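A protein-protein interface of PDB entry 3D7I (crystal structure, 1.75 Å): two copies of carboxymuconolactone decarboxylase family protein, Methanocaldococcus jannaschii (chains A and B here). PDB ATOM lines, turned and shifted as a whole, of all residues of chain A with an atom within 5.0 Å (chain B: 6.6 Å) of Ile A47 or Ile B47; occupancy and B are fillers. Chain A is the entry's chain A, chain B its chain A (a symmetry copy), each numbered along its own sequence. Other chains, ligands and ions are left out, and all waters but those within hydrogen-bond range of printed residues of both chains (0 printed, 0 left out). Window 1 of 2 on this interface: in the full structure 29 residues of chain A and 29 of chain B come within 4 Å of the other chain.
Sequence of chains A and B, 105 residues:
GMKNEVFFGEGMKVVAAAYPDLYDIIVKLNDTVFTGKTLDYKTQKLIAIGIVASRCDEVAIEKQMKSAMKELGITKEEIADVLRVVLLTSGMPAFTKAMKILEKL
NZ of Lys B42 lies within salt-bridge range of OE2 of Glu B78, 2.8 Å away.
O of Val B85 lies within hydrogen-bond range of OG1 of Thr B89, 2.8 Å away.
OG1 of Thr B89 lies within hydrogen-bond range of O of Val B86, 3.3 Å away.
Ile A47 touches just these residues of chain B: Ile B47 and Val B82.
Printed residues of chain B within 4 Å of Gly A50: Ile B51.
Lys B42 touches none of the printed residues of chain A.
Printed residues of chain A within 4 Å of Ile B47: Ile A47 and Val A82.
Printed residues of chain A within 4 Å of Gly B50: Ile A51 (3.6 Å).
Leu B83 touches none of the printed residues of chain A.
The nearest residue of chain A that does not touch Ile B47 is Val A85 (4.1 Å).
The nearest printed residue of chain A that does not touch Val B82 is Gln A44 (5.2 Å).
Among the printed residues, pairs that only touch across the chains: Leu A39 with Leu B46 (3.8 Å), Leu A39 with Glu B78 (3.6 Å), Leu A39 with Val B82 (3.8 Å), Gln A44 with Val B85 (3.8 Å), Leu A46 with Leu B39 (3.8 Å), Ile A47 with Ile B47 (3.9 Å), Ile A47 with Val B82 (3.8 Å), Ala A48 with Val B85 (3.7 Å), Gly A50 with Ile B51 (3.6 Å), Ile A51 with Gly B50 (3.6 Å), Ile A51 with Ile B51 (3.9 Å), Ile A51 with Val B86 (3.96 Å), Ile A51 with Thr B89 (3.4 Å), Val A82 with Leu B39 (3.8 Å), Val A82 with Ile B47 (3.8 Å), Val A85 with Gln B44 (3.8 Å) and Val A85 with Ala B48 (3.7 Å).
Leu A39 touches Leu B46, and with the chains exchanged Leu A46 touches Leu B39.
Ile A47 touches Val B82, and with the chains exchanged Val A82 touches Ile B47.
Ala A48 touches Val B85, and with the chains exchanged Val A85 touches Ala B48.
Gly A50 touches Ile B51, and with the chains exchanged Ile A51 touches Gly B50.
Positions printed for both chains: 39, 43, 44, 45, 46, 47, 48, 49, 50, 51, 82 and 85.
Printed residues of chain B that touch a printed residue of chain A: Leu B39, Gln B44, Leu B46, Ile B47, Ala B48, Gly B50, Ile B51, Glu B78, Asp B81, Val B82, Val B85, Val B86 and Thr B89.
Hydrophobic or aromatic side chains of chain B within 4 Å of the printed part of chain A: Leu B39, Leu B46, Ile B47, Ala B48, Ile B51, Val B82, Val B85 and Val B86.
Along chain B the printed residues that touch a printed residue of chain A span positions 39 to 89.
Hydrophobic or aromatic side chains of chain A that line the printed part of chain B: Leu A39, Leu A46, Ile A47, Ala A48, Ile A51, Val A82 and Val A85.
Along chain A the printed residues that touch a printed residue of chain B span positions 39 to 85.
Among the printed residues, 19 pairs touch across the chains.
Among the printed residues, no Asp or Glu carboxylate lies within 4 Å of a Lys or Arg side-chain nitrogen of the other chain.
OD2 of Asp B81 lies within hydrogen-bond range of N of Leu A39 (2.8 Å).
NE2 of Gln A44 is in hydrogen-bond range of O of Asp B81 (3.2 Å).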
ATOM      1  N   LEU A  39       7.808   1.358  26.666  1.00  0.00           N
ATOM      2  CA  LEU A  39       8.180   0.171  27.383  1.00  0.00           C
ATOM      3  C   LEU A  39       9.573   0.332  27.976  1.00  0.00           C
ATOM      4  O   LEU A  39      10.446   0.897  27.331  1.00  0.00           O
ATOM      5  CB  LEU A  39       8.159  -1.057  26.459  1.00  0.00           C
ATOM      6  CG  LEU A  39       6.814  -1.394  25.825  1.00  0.00           C
ATOM      7  CD1 LEU A  39       6.964  -2.753  25.051  1.00  0.00           C
ATOM      8  CD2 LEU A  39       5.712  -1.451  26.881  1.00  0.00           C
ATOM      9  N   THR A  43      11.102  -4.993  30.310  1.00  0.00           N
ATOM     10  CA  THR A  43      10.058  -5.553  29.442  1.00  0.00           C
ATOM     11  C   THR A  43      10.598  -5.947  28.083  1.00  0.00           C
ATOM     12  O   THR A  43      10.335  -7.045  27.591  1.00  0.00           O
ATOM     13  CB  THR A  43       8.892  -4.569  29.303  1.00  0.00           C
ATOM     14  OG1 THR A  43       8.336  -4.322  30.597  1.00  0.00           O
ATOM     15  CG2 THR A  43       7.782  -5.110  28.394  1.00  0.00           C
ATOM     16  N   GLN A  44      11.328  -5.045  27.455  1.00  0.00           N
ATOM     17  CA  GLN A  44      11.998  -5.361  26.178  1.00  0.00           C
ATOM     18  C   GLN A  44      12.944  -6.580  26.227  1.00  0.00           C
ATOM     19  O   GLN A  44      12.967  -7.414  25.296  1.00  0.00           O
ATOM     20  CB  GLN A  44      12.711  -4.127  25.674  1.00  0.00           C
ATOM     21  CG  GLN A  44      11.781  -3.027  25.196  1.00  0.00           C
ATOM     22  CD  GLN A  44      12.571  -1.913  24.568  1.00  0.00           C
ATOM     23  OE1 GLN A  44      13.465  -1.363  25.209  1.00  0.00           O
ATOM     24  NE2 GLN A  44      12.282  -1.603  23.293  1.00  0.00           N
ATOM     25  N   LYS A  45      13.694  -6.707  27.310  1.00  0.00           N
ATOM     26  CA  LYS A  45      14.608  -7.827  27.444  1.00  0.00           C
ATOM     27  C   LYS A  45      13.802  -9.156  27.634  1.00  0.00           C
ATOM     28  O   LYS A  45      14.204 -10.194  27.133  1.00  0.00           O
ATOM     29  CB  LYS A  45      15.631  -7.516  28.560  1.00  0.00           C
ATOM     30  CG  LYS A  45      17.092  -8.035  28.391  1.00  0.00           C
ATOM     31  CD  LYS A  45      17.820  -7.755  27.043  1.00  0.00           C
ATOM     32  CE  LYS A  45      18.675  -6.488  26.940  1.00  0.00           C
ATOM     33  NZ  LYS A  45      19.933  -6.765  26.117  1.00  0.00           N
ATOM     34  N   LEU A  46      12.673  -9.102  28.331  1.00  0.00           N
ATOM     35  CA  LEU A  46      11.793 -10.287  28.458  1.00  0.00           C
ATOM     36  C   LEU A  46      11.216 -10.700  27.087  1.00  0.00           C
ATOM     37  O   LEU A  46      11.151 -11.892  26.762  1.00  0.00           O
ATOM     38  CB  LEU A  46      10.687 -10.014  29.480  1.00  0.00           C
ATOM     39  CG  LEU A  46      11.155  -9.886  30.933  1.00  0.00           C
ATOM     40  CD1 LEU A  46      10.047  -9.229  31.762  1.00  0.00           C
ATOM     41  CD2 LEU A  46      11.597 -11.244  31.512  1.00  0.00           C
ATOM     42  N   ILE A  47      10.839  -9.699  26.293  1.00  0.00           N
ATOM     43  CA  ILE A  47      10.392  -9.922  24.920  1.00  0.00           C
ATOM     44  C   ILE A  47      11.503 -10.616  24.103  1.00  0.00           C
ATOM     45  O   ILE A  47      11.265 -11.590  23.379  1.00  0.00           O
ATOM     46  CB  ILE A  47       9.923  -8.624  24.233  1.00  0.00           C
ATOM     47  CG1 ILE A  47       8.659  -8.064  24.927  1.00  0.00           C
ATOM     48  CG2 ILE A  47       9.619  -8.896  22.746  1.00  0.00           C
ATOM     49  CD1 ILE A  47       8.382  -6.547  24.589  1.00  0.00           C
ATOM     50  N   ALA A  48      12.726 -10.131  24.260  1.00  0.00           N
ATOM     51  CA  ALA A  48      13.883 -10.723  23.542  1.00  0.00           C
ATOM     52  C   ALA A  48      14.070 -12.189  23.898  1.00  0.00           C
ATOM     53  O   ALA A  48      14.321 -13.020  23.034  1.00  0.00           O
ATOM     54  CB  ALA A  48      15.147  -9.943  23.852  1.00  0.00           C
ATOM     55  N   ILE A  49      13.972 -12.482  25.199  1.00  0.00           N
ATOM     56  CA  ILE A  49      14.014 -13.881  25.670  1.00  0.00           C
ATOM     57  C   ILE A  49      12.943 -14.719  24.967  1.00  0.00           C
ATOM     58  O   ILE A  49      13.213 -15.810  24.488  1.00  0.00           O
ATOM     59  CB  ILE A  49      13.915 -13.967  27.203  1.00  0.00           C
ATOM     60  CG1 ILE A  49      15.156 -13.371  27.841  1.00  0.00           C
ATOM     61  CG2 ILE A  49      13.782 -15.469  27.662  1.00  0.00           C
ATOM     62  CD1 ILE A  49      15.006 -13.046  29.371  1.00  0.00           C
ATOM     63  N   GLY A  50      11.715 -14.211  24.902  1.00  0.00           N
ATOM     64  CA  GLY A  50      10.624 -14.932  24.316  1.00  0.00           C
ATOM     65  C   GLY A  50      10.881 -15.248  22.865  1.00  0.00           C
ATOM     66  O   GLY A  50      10.661 -16.363  22.366  1.00  0.00           O
ATOM     67  N   ILE A  51      11.375 -14.251  22.145  1.00  0.00           N
ATOM     68  CA  ILE A  51      11.625 -14.441  20.722  1.00  0.00           C
ATOM     69  C   ILE A  51      12.715 -15.485  20.464  1.00  0.00           C
ATOM     70  O   ILE A  51      12.507 -16.422  19.719  1.00  0.00           O
ATOM     71  CB  ILE A  51      11.981 -13.113  20.024  1.00  0.00           C
ATOM     72  CG1 ILE A  51      10.754 -12.183  20.021  1.00  0.00           C
ATOM     73  CG2 ILE A  51      12.493 -13.412  18.579  1.00  0.00           C
ATOM     74  CD1 ILE A  51      11.084 -10.725  19.620  1.00  0.00           C
ATOM     75  N   VAL A  82       7.709 -15.993  30.777  1.00  0.00           N
ATOM     76  CA  VAL A  82       7.971 -15.807  29.354  1.00  0.00           C
ATOM     77  C   VAL A  82       7.782 -17.107  28.585  1.00  0.00           C
ATOM     78  O   VAL A  82       7.124 -17.138  27.552  1.00  0.00           O
ATOM     79  CB  VAL A  82       9.390 -15.235  29.086  1.00  0.00           C
ATOM     80  CG1 VAL A  82       9.670 -15.070  27.576  1.00  0.00           C
ATOM     81  CG2 VAL A  82       9.624 -13.854  29.838  1.00  0.00           C
ATOM     82  N   VAL A  85       4.365 -18.229  27.452  1.00  0.00           N
ATOM     83  CA  VAL A  85       3.980 -17.634  26.173  1.00  0.00           C
ATOM     84  C   VAL A  85       4.623 -18.353  25.015  1.00  0.00           C
ATOM     85  O   VAL A  85       4.001 -18.569  23.970  1.00  0.00           O
ATOM     86  CB  VAL A  85       4.284 -16.122  26.165  1.00  0.00           C
ATOM     87  CG1 VAL A  85       3.720 -15.490  24.878  1.00  0.00           C
ATOM     88  CG2 VAL A  85       3.658 -15.417  27.413  1.00  0.00           C
ATOM     89  N   LEU B  39       4.918 -12.074  36.121  1.00  0.00           N
ATOM     90  CA  LEU B  39       4.636 -11.148  35.061  1.00  0.00           C
ATOM     91  C   LEU B  39       3.131 -10.986  34.893  1.00  0.00           C
ATOM     92  O   LEU B  39       2.399 -11.960  34.999  1.00  0.00           O
ATOM     93  CB  LEU B  39       5.247 -11.631  33.735  1.00  0.00           C
ATOM     94  CG  LEU B  39       6.762 -11.790  33.715  1.00  0.00           C
ATOM     95  CD1 LEU B  39       7.199 -12.137  32.247  1.00  0.00           C
ATOM     96  CD2 LEU B  39       7.450 -10.532  34.240  1.00  0.00           C
ATOM     97  N   LYS B  42      -0.538  -7.961  30.579  1.00  0.00           N
ATOM     98  CA  LYS B  42      -0.051  -7.024  29.571  1.00  0.00           C
ATOM     99  C   LYS B  42       1.356  -7.370  29.066  1.00  0.00           C
ATOM    100  O   LYS B  42       1.608  -7.440  27.858  1.00  0.00           O
ATOM    101  CB  LYS B  42      -0.105  -5.589  30.109  1.00  0.00           C
ATOM    102  CG  LYS B  42       0.337  -4.534  29.115  1.00  0.00           C
ATOM    103  CD  LYS B  42       0.243  -3.143  29.721  1.00  0.00           C
ATOM    104  CE  LYS B  42       0.618  -2.101  28.689  1.00  0.00           C
ATOM    105  NZ  LYS B  42       0.678  -0.707  29.233  1.00  0.00           N
ATOM    106  N   THR B  43       2.275  -7.613  29.991  1.00  0.00           N
ATOM    107  CA  THR B  43       3.644  -7.996  29.620  1.00  0.00           C
ATOM    108  C   THR B  43       3.676  -9.264  28.792  1.00  0.00           C
ATOM    109  O   THR B  43       4.338  -9.328  27.756  1.00  0.00           O
ATOM    110  CB  THR B  43       4.520  -8.135  30.869  1.00  0.00           C
ATOM    111  OG1 THR B  43       4.557  -6.880  31.551  1.00  0.00           O
ATOM    112  CG2 THR B  43       5.956  -8.545  30.527  1.00  0.00           C
ATOM    113  N   GLN B  44       2.988 -10.289  29.258  1.00  0.00           N
ATOM    114  CA  GLN B  44       2.857 -11.536  28.479  1.00  0.00           C
ATOM    115  C   GLN B  44       2.268 -11.357  27.063  1.00  0.00           C
ATOM    116  O   GLN B  44       2.745 -11.973  26.086  1.00  0.00           O
ATOM    117  CB  GLN B  44       2.064 -12.542  29.284  1.00  0.00           C
ATOM    118  CG  GLN B  44       2.805 -13.085  30.493  1.00  0.00           C
ATOM    119  CD  GLN B  44       2.010 -14.189  31.135  1.00  0.00           C
ATOM    120  OE1 GLN B  44       0.853 -13.977  31.496  1.00  0.00           O
ATOM    121  NE2 GLN B  44       2.605 -15.389  31.240  1.00  0.00           N
ATOM    122  N   LYS B  45       1.267 -10.500  26.940  1.00  0.00           N
ATOM    123  CA  LYS B  45       0.658 -10.263  25.643  1.00  0.00           C
ATOM    124  C   LYS B  45       1.657  -9.497  24.713  1.00  0.00           C
ATOM    125  O   LYS B  45       1.700  -9.748  23.519  1.00  0.00           O
ATOM    126  CB  LYS B  45      -0.710  -9.573  25.845  1.00  0.00           C
ATOM    127  CG  LYS B  45      -1.870  -9.927  24.865  1.00  0.00           C
ATOM    128  CD  LYS B  45      -2.177 -11.432  24.603  1.00  0.00           C
ATOM    129  CE  LYS B  45      -3.234 -12.111  25.478  1.00  0.00           C
ATOM    130  NZ  LYS B  45      -4.059 -13.093  24.645  1.00  0.00           N
ATOM    131  N   LEU B  46       2.457  -8.596  25.272  1.00  0.00           N
ATOM    132  CA  LEU B  46       3.510  -7.913  24.485  1.00  0.00           C
ATOM    133  C   LEU B  46       4.576  -8.917  23.993  1.00  0.00           C
ATOM    134  O   LEU B  46       5.027  -8.846  22.842  1.00  0.00           O
ATOM    135  CB  LEU B  46       4.133  -6.784  25.308  1.00  0.00           C
ATOM    136  CG  LEU B  46       3.211  -5.593  25.590  1.00  0.00           C
ATOM    137  CD1 LEU B  46       3.804  -4.755  26.726  1.00  0.00           C
ATOM    138  CD2 LEU B  46       2.950  -4.761  24.319  1.00  0.00           C
ATOM    139  N   ILE B  47       4.931  -9.857  24.866  1.00  0.00           N
ATOM    140  CA  ILE B  47       5.832 -10.950  24.508  1.00  0.00           C
ATOM    141  C   ILE B  47       5.242 -11.767  23.338  1.00  0.00           C
ATOM    142  O   ILE B  47       5.925 -12.087  22.359  1.00  0.00           O
ATOM    143  CB  ILE B  47       6.166 -11.859  25.708  1.00  0.00           C
ATOM    144  CG1 ILE B  47       6.969 -11.079  26.776  1.00  0.00           C
ATOM    145  CG2 ILE B  47       6.985 -13.077  25.234  1.00  0.00           C
ATOM    146  CD1 ILE B  47       6.964 -11.776  28.193  1.00  0.00           C
ATOM    147  N   ALA B  48       3.953 -12.062  23.431  1.00  0.00           N
ATOM    148  CA  ALA B  48       3.263 -12.828  22.362  1.00  0.00           C
ATOM    149  C   ALA B  48       3.334 -12.109  21.026  1.00  0.00           C
ATOM    150  O   ALA B  48       3.579 -12.720  19.993  1.00  0.00           O
ATOM    151  CB  ALA B  48       1.817 -13.081  22.747  1.00  0.00           C
ATOM    152  N   ILE B  49       3.081 -10.796  21.065  1.00  0.00           N
ATOM    153  CA  ILE B  49       3.230  -9.954  19.861  1.00  0.00           C
ATOM    154  C   ILE B  49       4.639 -10.094  19.277  1.00  0.00           C
ATOM    155  O   ILE B  49       4.807 -10.277  18.081  1.00  0.00           O
ATOM    156  CB  ILE B  49       2.854  -8.489  20.142  1.00  0.00           C
ATOM    157  CG1 ILE B  49       1.370  -8.378  20.435  1.00  0.00           C
ATOM    158  CG2 ILE B  49       3.193  -7.586  18.896  1.00  0.00           C
ATOM    159  CD1 ILE B  49       0.943  -7.025  21.111  1.00  0.00           C
ATOM    160  N   GLY B  50       5.663 -10.009  20.123  1.00  0.00           N
ATOM    161  CA  GLY B  50       7.022 -10.072  19.678  1.00  0.00           C
ATOM    162  C   GLY B  50       7.326 -11.380  18.993  1.00  0.00           C
ATOM    163  O   GLY B  50       7.955 -11.455  17.927  1.00  0.00           O
ATOM    164  N   ILE B  51       6.860 -12.461  19.602  1.00  0.00           N
ATOM    165  CA  ILE B  51       7.130 -13.779  19.041  1.00  0.00           C
ATOM    166  C   ILE B  51       6.465 -13.970  17.675  1.00  0.00           C
ATOM    167  O   ILE B  51       7.119 -14.329  16.716  1.00  0.00           O
ATOM    168  CB  ILE B  51       6.705 -14.905  20.005  1.00  0.00           C
ATOM    169  CG1 ILE B  51       7.604 -14.888  21.254  1.00  0.00           C
ATOM    170  CG2 ILE B  51       6.767 -16.274  19.255  1.00  0.00           C
ATOM    171  CD1 ILE B  51       7.078 -15.772  22.408  1.00  0.00           C
ATOM    172  N   VAL B  52       5.179 -13.694  17.582  1.00  0.00           N
ATOM    173  CA  VAL B  52       4.504 -13.860  16.275  1.00  0.00           C
ATOM    174  C   VAL B  52       4.996 -12.854  15.236  1.00  0.00           C
ATOM    175  O   VAL B  52       5.141 -13.215  14.074  1.00  0.00           O
ATOM    176  CB  VAL B  52       2.959 -13.877  16.355  1.00  0.00           C
ATOM    177  CG1 VAL B  52       2.498 -15.108  17.168  1.00  0.00           C
ATOM    178  CG2 VAL B  52       2.360 -12.518  16.876  1.00  0.00           C
ATOM    179  N   GLU B  78       3.518   1.479  21.971  1.00  0.00           N
ATOM    180  CA  GLU B  78       3.928   0.339  22.786  1.00  0.00           C
ATOM    181  C   GLU B  78       4.239  -0.862  21.903  1.00  0.00           C
ATOM    182  O   GLU B  78       5.242  -1.555  22.112  1.00  0.00           O
ATOM    183  CB  GLU B  78       2.867  -0.029  23.832  1.00  0.00           C
ATOM    184  CG  GLU B  78       2.672   0.982  24.931  1.00  0.00           C
ATOM    185  CD  GLU B  78       1.620   0.536  25.931  1.00  0.00           C
ATOM    186  OE1 GLU B  78       0.557   0.039  25.498  1.00  0.00           O
ATOM    187  OE2 GLU B  78       1.861   0.662  27.153  1.00  0.00           O
ATOM    188  N   ASP B  81       7.579  -0.445  20.257  1.00  0.00           N
ATOM    189  CA  ASP B  81       8.667  -0.777  21.183  1.00  0.00           C
ATOM    190  C   ASP B  81       8.943  -2.270  21.167  1.00  0.00           C
ATOM    191  O   ASP B  81      10.089  -2.691  21.301  1.00  0.00           O
ATOM    192  CB  ASP B  81       8.372  -0.332  22.612  1.00  0.00           C
ATOM    193  CG  ASP B  81       8.502   1.179  22.828  1.00  0.00           C
ATOM    194  OD1 ASP B  81       9.058   1.874  21.955  1.00  0.00           O
ATOM    195  OD2 ASP B  81       8.031   1.631  23.887  1.00  0.00           O
ATOM    196  N   VAL B  82       7.896  -3.085  21.013  1.00  0.00           N
ATOM    197  CA  VAL B  82       8.064  -4.517  20.796  1.00  0.00           C
ATOM    198  C   VAL B  82       8.796  -4.794  19.490  1.00  0.00           C
ATOM    199  O   VAL B  82       9.735  -5.580  19.449  1.00  0.00           O
ATOM    200  CB  VAL B  82       6.710  -5.278  20.814  1.00  0.00           C
ATOM    201  CG1 VAL B  82       6.894  -6.790  20.554  1.00  0.00           C
ATOM    202  CG2 VAL B  82       5.923  -5.052  22.177  1.00  0.00           C
ATOM    203  N   LEU B  83       8.369  -4.111  18.438  1.00  0.00           N
ATOM    204  CA  LEU B  83       8.959  -4.283  17.116  1.00  0.00           C
ATOM    205  C   LEU B  83      10.424  -3.876  17.038  1.00  0.00           C
ATOM    206  O   LEU B  83      11.189  -4.464  16.289  1.00  0.00           O
ATOM    207  CB  LEU B  83       8.101  -3.591  16.063  1.00  0.00           C
ATOM    208  CG  LEU B  83       6.659  -4.073  15.948  1.00  0.00           C
ATOM    209  CD1 LEU B  83       5.986  -3.427  14.685  1.00  0.00           C
ATOM    210  CD2 LEU B  83       6.540  -5.624  15.915  1.00  0.00           C
ATOM    211  N   VAL B  85      12.562  -4.680  19.297  1.00  0.00           N
ATOM    212  CA  VAL B  85      13.176  -5.945  19.695  1.00  0.00           C
ATOM    213  C   VAL B  85      13.129  -6.956  18.578  1.00  0.00           C
ATOM    214  O   VAL B  85      14.085  -7.705  18.352  1.00  0.00           O
ATOM    215  CB  VAL B  85      12.534  -6.477  20.992  1.00  0.00           C
ATOM    216  CG1 VAL B  85      13.308  -7.717  21.479  1.00  0.00           C
ATOM    217  CG2 VAL B  85      12.542  -5.383  22.110  1.00  0.00           C
ATOM    218  N   VAL B  86      12.023  -6.975  17.822  1.00  0.00           N
ATOM    219  CA  VAL B  86      11.907  -7.882  16.658  1.00  0.00           C
ATOM    220  C   VAL B  86      13.026  -7.610  15.644  1.00  0.00           C
ATOM    221  O   VAL B  86      13.680  -8.538  15.169  1.00  0.00           O
ATOM    222  CB  VAL B  86      10.521  -7.740  16.003  1.00  0.00           C
ATOM    223  CG1 VAL B  86      10.455  -8.539  14.700  1.00  0.00           C
ATOM    224  CG2 VAL B  86       9.400  -8.227  17.046  1.00  0.00           C
ATOM    225  N   THR B  89      16.436  -8.918  17.014  1.00  0.00           N
ATOM    226  CA  THR B  89      16.492 -10.368  17.167  1.00  0.00           C
ATOM    227  C   THR B  89      16.238 -11.110  15.877  1.00  0.00           C
ATOM    228  O   THR B  89      16.591 -12.275  15.738  1.00  0.00           O
ATOM    229  CB  THR B  89      15.450 -10.885  18.187  1.00  0.00           C
ATOM    230  OG1 THR B  89      14.129 -10.489  17.756  1.00  0.00           O
ATOM    231  CG2 THR B  89      15.730 -10.350  19.614  1.00  0.00           C
